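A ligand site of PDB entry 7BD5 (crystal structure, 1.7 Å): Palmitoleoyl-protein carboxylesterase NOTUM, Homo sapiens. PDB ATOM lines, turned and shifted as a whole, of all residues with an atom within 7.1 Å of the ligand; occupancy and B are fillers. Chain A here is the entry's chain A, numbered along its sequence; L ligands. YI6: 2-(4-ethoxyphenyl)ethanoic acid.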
ATOM      1  N   GLU A  48      19.569 -19.174  17.313  1.00  0.00           N
ATOM      2  CA  GLU A  48      19.436 -20.616  17.112  1.00  0.00           C
ATOM      3  C   GLU A  48      20.782 -21.255  16.776  1.00  0.00           C
ATOM      4  O   GLU A  48      21.664 -20.612  16.182  1.00  0.00           O
ATOM      5  CB  GLU A  48      18.436 -20.893  15.996  1.00  0.00           C
ATOM      6  CG  GLU A  48      18.043 -22.382  15.783  1.00  0.00           C
ATOM      7  CD  GLU A  48      17.162 -22.605  14.563  1.00  0.00           C
ATOM      8  OE1 GLU A  48      17.180 -21.734  13.645  1.00  0.00           O
ATOM      9  OE2 GLU A  48      16.456 -23.635  14.505  1.00  0.00           O
ATOM     10  N   GLY A  49      20.918 -22.552  17.100  1.00  0.00           N
ATOM     11  CA  GLY A  49      22.072 -23.345  16.731  1.00  0.00           C
ATOM     12  C   GLY A  49      21.760 -24.350  15.633  1.00  0.00           C
ATOM     13  O   GLY A  49      20.718 -24.296  14.978  1.00  0.00           O
ATOM     14  N   GLY A  50      22.712 -25.287  15.444  1.00  0.00           N
ATOM     15  CA  GLY A  50      22.573 -26.344  14.443  1.00  0.00           C
ATOM     16  C   GLY A  50      23.819 -26.630  13.592  1.00  0.00           C
ATOM     17  O   GLY A  50      23.708 -26.740  12.361  1.00  0.00           O
ATOM     18  N   TRP A  51      24.989 -26.798  14.221  1.00  0.00           N
ATOM     19  CA  TRP A  51      26.257 -27.208  13.549  1.00  0.00           C
ATOM     20  C   TRP A  51      26.632 -26.149  12.509  1.00  0.00           C
ATOM     21  O   TRP A  51      26.448 -24.951  12.770  1.00  0.00           O
ATOM     22  CB  TRP A  51      26.133 -28.640  13.004  1.00  0.00           C
ATOM     23  CG  TRP A  51      26.094 -29.652  14.119  1.00  0.00           C
ATOM     24  CD1 TRP A  51      24.986 -30.194  14.697  1.00  0.00           C
ATOM     25  CD2 TRP A  51      27.225 -30.217  14.819  1.00  0.00           C
ATOM     26  NE1 TRP A  51      25.348 -31.069  15.706  1.00  0.00           N
ATOM     27  CE2 TRP A  51      26.717 -31.088  15.801  1.00  0.00           C
ATOM     28  CE3 TRP A  51      28.609 -30.074  14.694  1.00  0.00           C
ATOM     29  CZ2 TRP A  51      27.548 -31.825  16.652  1.00  0.00           C
ATOM     30  CZ3 TRP A  51      29.440 -30.787  15.551  1.00  0.00           C
ATOM     31  CH2 TRP A  51      28.902 -31.658  16.510  1.00  0.00           C
ATOM     32  N   TYR A  52      27.208 -26.537  11.362  1.00  0.00           N
ATOM     33  CA  TYR A  52      27.689 -25.629  10.311  1.00  0.00           C
ATOM     34  C   TYR A  52      28.064 -26.482   9.101  1.00  0.00           C
ATOM     35  O   TYR A  52      27.990 -27.707   9.145  1.00  0.00           O
ATOM     36  CB  TYR A  52      28.874 -24.771  10.787  1.00  0.00           C
ATOM     37  CG  TYR A  52      30.105 -25.547  11.279  1.00  0.00           C
ATOM     38  CD1 TYR A  52      30.286 -25.815  12.634  1.00  0.00           C
ATOM     39  CD2 TYR A  52      31.070 -25.979  10.392  1.00  0.00           C
ATOM     40  CE1 TYR A  52      31.413 -26.510  13.091  1.00  0.00           C
ATOM     41  CE2 TYR A  52      32.196 -26.682  10.828  1.00  0.00           C
ATOM     42  CZ  TYR A  52      32.365 -26.932  12.177  1.00  0.00           C
ATOM     43  OH  TYR A  52      33.480 -27.616  12.606  1.00  0.00           O
ATOM     44  N   TYR A 105      18.757 -19.550  12.511  1.00  0.00           N
ATOM     45  CA  TYR A 105      20.121 -19.809  12.031  1.00  0.00           C
ATOM     46  C   TYR A 105      19.988 -20.345  10.608  1.00  0.00           C
ATOM     47  O   TYR A 105      19.571 -21.476  10.400  1.00  0.00           O
ATOM     48  CB  TYR A 105      20.794 -20.815  12.954  1.00  0.00           C
ATOM     49  CG  TYR A 105      22.227 -21.254  12.663  1.00  0.00           C
ATOM     50  CD1 TYR A 105      23.202 -20.339  12.244  1.00  0.00           C
ATOM     51  CD2 TYR A 105      22.609 -22.572  12.891  1.00  0.00           C
ATOM     52  CE1 TYR A 105      24.534 -20.748  12.037  1.00  0.00           C
ATOM     53  CE2 TYR A 105      23.918 -22.978  12.689  1.00  0.00           C
ATOM     54  CZ  TYR A 105      24.876 -22.064  12.252  1.00  0.00           C
ATOM     55  OH  TYR A 105      26.173 -22.476  12.038  1.00  0.00           O
ATOM     56  N   VAL A 110      28.375 -20.528  12.138  1.00  0.00           N
ATOM     57  CA  VAL A 110      28.498 -20.207  13.551  1.00  0.00           C
ATOM     58  C   VAL A 110      28.301 -18.707  13.790  1.00  0.00           C
ATOM     59  O   VAL A 110      28.874 -18.118  14.720  1.00  0.00           O
ATOM     60  CB  VAL A 110      29.834 -20.734  14.130  1.00  0.00           C
ATOM     61  CG1 VAL A 110      29.744 -20.860  15.656  1.00  0.00           C
ATOM     62  CG2 VAL A 110      30.217 -22.109  13.528  1.00  0.00           C
ATOM     63  N   SER A 154      21.972 -20.802  21.874  1.00  0.00           N
ATOM     64  CA  SER A 154      22.243 -22.189  22.248  1.00  0.00           C
ATOM     65  C   SER A 154      23.039 -22.917  21.161  1.00  0.00           C
ATOM     66  O   SER A 154      22.770 -22.753  19.965  1.00  0.00           O
ATOM     67  CB  SER A 154      20.934 -22.966  22.504  1.00  0.00           C
ATOM     68  OG  SER A 154      20.226 -22.474  23.642  1.00  0.00           O
ATOM     69  N   SER A 155      24.007 -23.732  21.605  1.00  0.00           N
ATOM     70  CA  SER A 155      24.826 -24.603  20.742  1.00  0.00           C
ATOM     71  C   SER A 155      25.643 -23.716  19.801  1.00  0.00           C
ATOM     72  O   SER A 155      26.398 -22.862  20.292  1.00  0.00           O
ATOM     73  CB  SER A 155      23.920 -25.631  20.066  1.00  0.00           C
ATOM     74  OG  SER A 155      23.070 -26.277  20.995  1.00  0.00           O
ATOM     75  N   ALA A 156      25.560 -23.879  18.474  1.00  0.00           N
ATOM     76  CA  ALA A 156      26.309 -22.960  17.611  1.00  0.00           C
ATOM     77  C   ALA A 156      25.881 -21.515  17.839  1.00  0.00           C
ATOM     78  O   ALA A 156      26.667 -20.591  17.614  1.00  0.00           O
ATOM     79  CB  ALA A 156      26.148 -23.364  16.140  1.00  0.00           C
ATOM     80  N   GLY A 157      24.640 -21.292  18.303  1.00  0.00           N
ATOM     81  CA  GLY A 157      24.228 -19.957  18.668  1.00  0.00           C
ATOM     82  C   GLY A 157      24.853 -19.441  19.949  1.00  0.00           C
ATOM     83  O   GLY A 157      24.988 -18.232  20.147  1.00  0.00           O
ATOM     84  N   GLY A 158      25.189 -20.351  20.872  1.00  0.00           N
ATOM     85  CA  GLY A 158      25.938 -19.933  22.054  1.00  0.00           C
ATOM     86  C   GLY A 158      27.331 -19.460  21.689  1.00  0.00           C
ATOM     87  O   GLY A 158      27.809 -18.445  22.191  1.00  0.00           O
ATOM     88  N   THR A 159      28.017 -20.193  20.800  1.00  0.00           N
ATOM     89  CA  THR A 159      29.290 -19.693  20.307  1.00  0.00           C
ATOM     90  C   THR A 159      29.096 -18.363  19.572  1.00  0.00           C
ATOM     91  O   THR A 159      29.924 -17.455  19.694  1.00  0.00           O
ATOM     92  CB  THR A 159      29.957 -20.735  19.397  1.00  0.00           C
ATOM     93  OG1 THR A 159      29.964 -22.013  20.074  1.00  0.00           O
ATOM     94  CG2 THR A 159      31.387 -20.334  19.109  1.00  0.00           C
ATOM     95  N   GLY A 160      27.980 -18.234  18.839  1.00  0.00           N
ATOM     96  CA  GLY A 160      27.681 -16.981  18.163  1.00  0.00           C
ATOM     97  C   GLY A 160      27.543 -15.800  19.098  1.00  0.00           C
ATOM     98  O   GLY A 160      27.906 -14.669  18.744  1.00  0.00           O
ATOM     99  N   SER A 188      25.621 -23.784  25.976  1.00  0.00           N
ATOM    100  CA  SER A 188      26.114 -24.964  25.275  1.00  0.00           C
ATOM    101  C   SER A 188      27.016 -24.611  24.091  1.00  0.00           C
ATOM    102  O   SER A 188      27.020 -25.321  23.081  1.00  0.00           O
ATOM    103  CB  SER A 188      24.945 -25.855  24.834  1.00  0.00           C
ATOM    104  OG  SER A 188      24.186 -26.257  25.963  1.00  0.00           O
ATOM    105  N   GLY A 189      27.782 -23.526  24.226  1.00  0.00           N
ATOM    106  CA  GLY A 189      28.686 -23.079  23.164  1.00  0.00           C
ATOM    107  C   GLY A 189      30.140 -22.968  23.592  1.00  0.00           C
ATOM    108  O   GLY A 189      30.934 -22.282  22.934  1.00  0.00           O
ATOM    109  N   TRP A 190      30.512 -23.637  24.677  1.00  0.00           N
ATOM    110  CA  TRP A 190      31.812 -23.492  25.354  1.00  0.00           C
ATOM    111  C   TRP A 190      32.547 -24.827  25.230  1.00  0.00           C
ATOM    112  O   TRP A 190      32.369 -25.727  26.062  1.00  0.00           O
ATOM    113  CB  TRP A 190      31.569 -23.102  26.827  1.00  0.00           C
ATOM    114  CG  TRP A 190      32.801 -22.799  27.673  1.00  0.00           C
ATOM    115  CD1 TRP A 190      33.564 -23.697  28.364  1.00  0.00           C
ATOM    116  CD2 TRP A 190      33.321 -21.486  27.989  1.00  0.00           C
ATOM    117  NE1 TRP A 190      34.568 -23.020  29.062  1.00  0.00           N
ATOM    118  CE2 TRP A 190      34.422 -21.676  28.846  1.00  0.00           C
ATOM    119  CE3 TRP A 190      32.950 -20.188  27.629  1.00  0.00           C
ATOM    120  CZ2 TRP A 190      35.181 -20.595  29.346  1.00  0.00           C
ATOM    121  CZ3 TRP A 190      33.697 -19.112  28.118  1.00  0.00           C
ATOM    122  CH2 TRP A 190      34.799 -19.327  28.969  1.00  0.00           C
ATOM    123  N   PHE A 191      33.387 -24.943  24.192  1.00  0.00           N
ATOM    124  CA  PHE A 191      34.035 -26.195  23.827  1.00  0.00           C
ATOM    125  C   PHE A 191      35.538 -26.187  24.086  1.00  0.00           C
ATOM    126  O   PHE A 191      36.185 -25.136  24.192  1.00  0.00           O
ATOM    127  CB  PHE A 191      33.746 -26.500  22.354  1.00  0.00           C
ATOM    128  CG  PHE A 191      32.289 -26.700  22.079  1.00  0.00           C
ATOM    129  CD1 PHE A 191      31.552 -25.709  21.461  1.00  0.00           C
ATOM    130  CD2 PHE A 191      31.635 -27.827  22.547  1.00  0.00           C
ATOM    131  CE1 PHE A 191      30.208 -25.881  21.232  1.00  0.00           C
ATOM    132  CE2 PHE A 191      30.272 -28.001  22.329  1.00  0.00           C
ATOM    133  CZ  PHE A 191      29.564 -27.017  21.669  1.00  0.00           C
ATOM    134  N   ILE A 214      36.954 -25.904  11.350  1.00  0.00           N
ATOM    135  CA  ILE A 214      36.695 -24.495  11.603  1.00  0.00           C
ATOM    136  C   ILE A 214      37.666 -23.617  10.825  1.00  0.00           C
ATOM    137  O   ILE A 214      37.286 -22.584  10.264  1.00  0.00           O
ATOM    138  CB  ILE A 214      36.775 -24.195  13.123  1.00  0.00           C
ATOM    139  CG1 ILE A 214      35.622 -24.880  13.852  1.00  0.00           C
ATOM    140  CG2 ILE A 214      36.799 -22.685  13.371  1.00  0.00           C
ATOM    141  CD1 ILE A 214      35.722 -24.763  15.367  1.00  0.00           C
ATOM    142  N   PHE A 242      37.033 -19.171  18.288  1.00  0.00           N
ATOM    143  CA  PHE A 242      35.788 -19.931  18.376  1.00  0.00           C
ATOM    144  C   PHE A 242      35.736 -20.794  19.627  1.00  0.00           C
ATOM    145  O   PHE A 242      34.729 -21.476  19.845  1.00  0.00           O
ATOM    146  CB  PHE A 242      35.611 -20.823  17.137  1.00  0.00           C
ATOM    147  CG  PHE A 242      35.197 -20.089  15.897  1.00  0.00           C
ATOM    148  CD1 PHE A 242      36.035 -19.170  15.282  1.00  0.00           C
ATOM    149  CD2 PHE A 242      33.962 -20.355  15.295  1.00  0.00           C
ATOM    150  CE1 PHE A 242      35.643 -18.501  14.122  1.00  0.00           C
ATOM    151  CE2 PHE A 242      33.558 -19.701  14.146  1.00  0.00           C
ATOM    152  CZ  PHE A 242      34.397 -18.774  13.553  1.00  0.00           C
ATOM    153  N   PHE A 243      36.785 -20.802  20.451  1.00  0.00           N
ATOM    154  CA  PHE A 243      36.820 -21.615  21.651  1.00  0.00           C
ATOM    155  C   PHE A 243      36.641 -20.710  22.864  1.00  0.00           C
ATOM    156  O   PHE A 243      37.467 -19.831  23.098  1.00  0.00           O
ATOM    157  CB  PHE A 243      38.118 -22.425  21.702  1.00  0.00           C
ATOM    158  CG  PHE A 243      38.081 -23.573  20.715  1.00  0.00           C
ATOM    159  CD1 PHE A 243      38.450 -23.381  19.399  1.00  0.00           C
ATOM    160  CD2 PHE A 243      37.546 -24.791  21.077  1.00  0.00           C
ATOM    161  CE1 PHE A 243      38.363 -24.413  18.472  1.00  0.00           C
ATOM    162  CE2 PHE A 243      37.456 -25.833  20.159  1.00  0.00           C
ATOM    163  CZ  PHE A 243      37.849 -25.636  18.859  1.00  0.00           C
ATOM    164  N   ASP A 263      29.051 -32.352  27.825  1.00  0.00           N
ATOM    165  CA  ASP A 263      28.181 -31.975  26.728  1.00  0.00           C
ATOM    166  C   ASP A 263      28.234 -33.010  25.604  1.00  0.00           C
ATOM    167  O   ASP A 263      29.313 -33.489  25.226  1.00  0.00           O
ATOM    168  CB  ASP A 263      28.595 -30.599  26.198  1.00  0.00           C
ATOM    169  CG  ASP A 263      27.658 -30.083  25.148  1.00  0.00           C
ATOM    170  OD1 ASP A 263      26.636 -29.492  25.533  1.00  0.00           O
ATOM    171  OD2 ASP A 263      27.946 -30.272  23.961  1.00  0.00           O
ATOM    172  N   ALA A 265      27.621 -32.771  22.378  1.00  0.00           N
ATOM    173  CA  ALA A 265      28.274 -32.359  21.141  1.00  0.00           C
ATOM    174  C   ALA A 265      29.794 -32.411  21.293  1.00  0.00           C
ATOM    175  O   ALA A 265      30.507 -32.746  20.329  1.00  0.00           O
ATOM    176  CB  ALA A 265      27.823 -30.952  20.754  1.00  0.00           C
ATOM    177  N   GLN A 266      30.303 -32.052  22.466  1.00  0.00           N
ATOM    178  CA  GLN A 266      31.731 -32.226  22.764  1.00  0.00           C
ATOM    179  C   GLN A 266      32.125 -33.704  22.697  1.00  0.00           C
ATOM    180  O   GLN A 266      33.142 -34.061  22.076  1.00  0.00           O
ATOM    181  CB  GLN A 266      32.026 -31.639  24.154  1.00  0.00           C
ATOM    182  CG  GLN A 266      33.459 -31.865  24.629  1.00  0.00           C
ATOM    183  CD  GLN A 266      34.426 -30.821  24.099  1.00  0.00           C
ATOM    184  OE1 GLN A 266      34.203 -29.615  24.231  1.00  0.00           O
ATOM    185  NE2 GLN A 266      35.542 -31.294  23.517  1.00  0.00           N
ATOM    186  N   VAL A 269      32.294 -34.863  18.944  1.00  0.00           N
ATOM    187  CA  VAL A 269      33.510 -34.547  18.202  1.00  0.00           C
ATOM    188  C   VAL A 269      34.727 -35.253  18.792  1.00  0.00           C
ATOM    189  O   VAL A 269      35.717 -35.484  18.072  1.00  0.00           O
ATOM    190  CB  VAL A 269      33.688 -33.026  18.074  1.00  0.00           C
ATOM    191  CG1 VAL A 269      32.506 -32.407  17.337  1.00  0.00           C
ATOM    192  CG2 VAL A 269      33.879 -32.374  19.431  1.00  0.00           C
ATOM    193  N   HIS A 312      22.341 -32.815  25.859  1.00  0.00           N
ATOM    194  CA  HIS A 312      22.350 -31.868  24.756  1.00  0.00           C
ATOM    195  C   HIS A 312      21.176 -30.895  24.809  1.00  0.00           C
ATOM    196  O   HIS A 312      20.897 -30.226  23.806  1.00  0.00           O
ATOM    197  CB  HIS A 312      22.345 -32.595  23.408  1.00  0.00           C
ATOM    198  CG  HIS A 312      21.016 -33.215  23.074  1.00  0.00           C
ATOM    199  ND1 HIS A 312      20.492 -34.264  23.798  1.00  0.00           N
ATOM    200  CD2 HIS A 312      20.121 -32.946  22.100  1.00  0.00           C
ATOM    201  CE1 HIS A 312      19.321 -34.603  23.283  1.00  0.00           C
ATOM    202  NE2 HIS A 312      19.079 -33.823  22.255  1.00  0.00           N
HETATM  203  C12 YI6 L   1      29.215 -25.260  18.188  1.00  0.00           C
HETATM  204  C13 YI6 L   1      28.134 -26.024  18.618  1.00  0.00           C
HETATM  205  C5  YI6 L   1      27.671 -27.094  17.878  1.00  0.00           C
HETATM  206  C6  YI6 L   1      28.303 -27.416  16.684  1.00  0.00           C
HETATM  207  C7  YI6 L   1      29.392 -26.665  16.254  1.00  0.00           C
HETATM  208  C8  YI6 L   1      29.855 -25.595  16.994  1.00  0.00           C
HETATM  209  C2  YI6 L   1      25.121 -27.590  17.699  1.00  0.00           C
HETATM  210  O9  YI6 L   1      30.969 -24.868  16.524  1.00  0.00           O
HETATM  211  C10 YI6 L   1      31.547 -24.000  17.444  1.00  0.00           C
HETATM  212  C11 YI6 L   1      32.865 -24.598  17.932  1.00  0.00           C
HETATM  213  O1  YI6 L   1      24.122 -28.346  17.878  1.00  0.00           O
HETATM  214  O3  YI6 L   1      24.995 -26.548  17.002  1.00  0.00           O
HETATM  215  C4  YI6 L   1      26.475 -27.938  18.325  1.00  0.00           C
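The side-chain hydroxyl of Tyr 105 lies within hydrogen-bond range of the backbone carbonyl oxygen of Trp 51, 2.6 Å away.
OG1 of Thr 159 lies within hydrogen-bond range of O of Gly 189 (3.0 Å).
O3 of the ligand lies within hydrogen-bond range of N of Trp 51 (2.8 Å).
O3 of the ligand lies within hydrogen-bond range of N of Gly 50 (3.0 Å).
N of Ala 156 is in hydrogen-bond range of O3 of the ligand (3.1 Å).
Merely in contact with the ligand: Phe 191, Ser 155, Thr 159, Tyr 52 and Ile 214.
Hydrophobic or aromatic side chains within 4 Å of the ligand: Trp 51, Tyr 52, Ala 156, Phe 191 and Ile 214.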
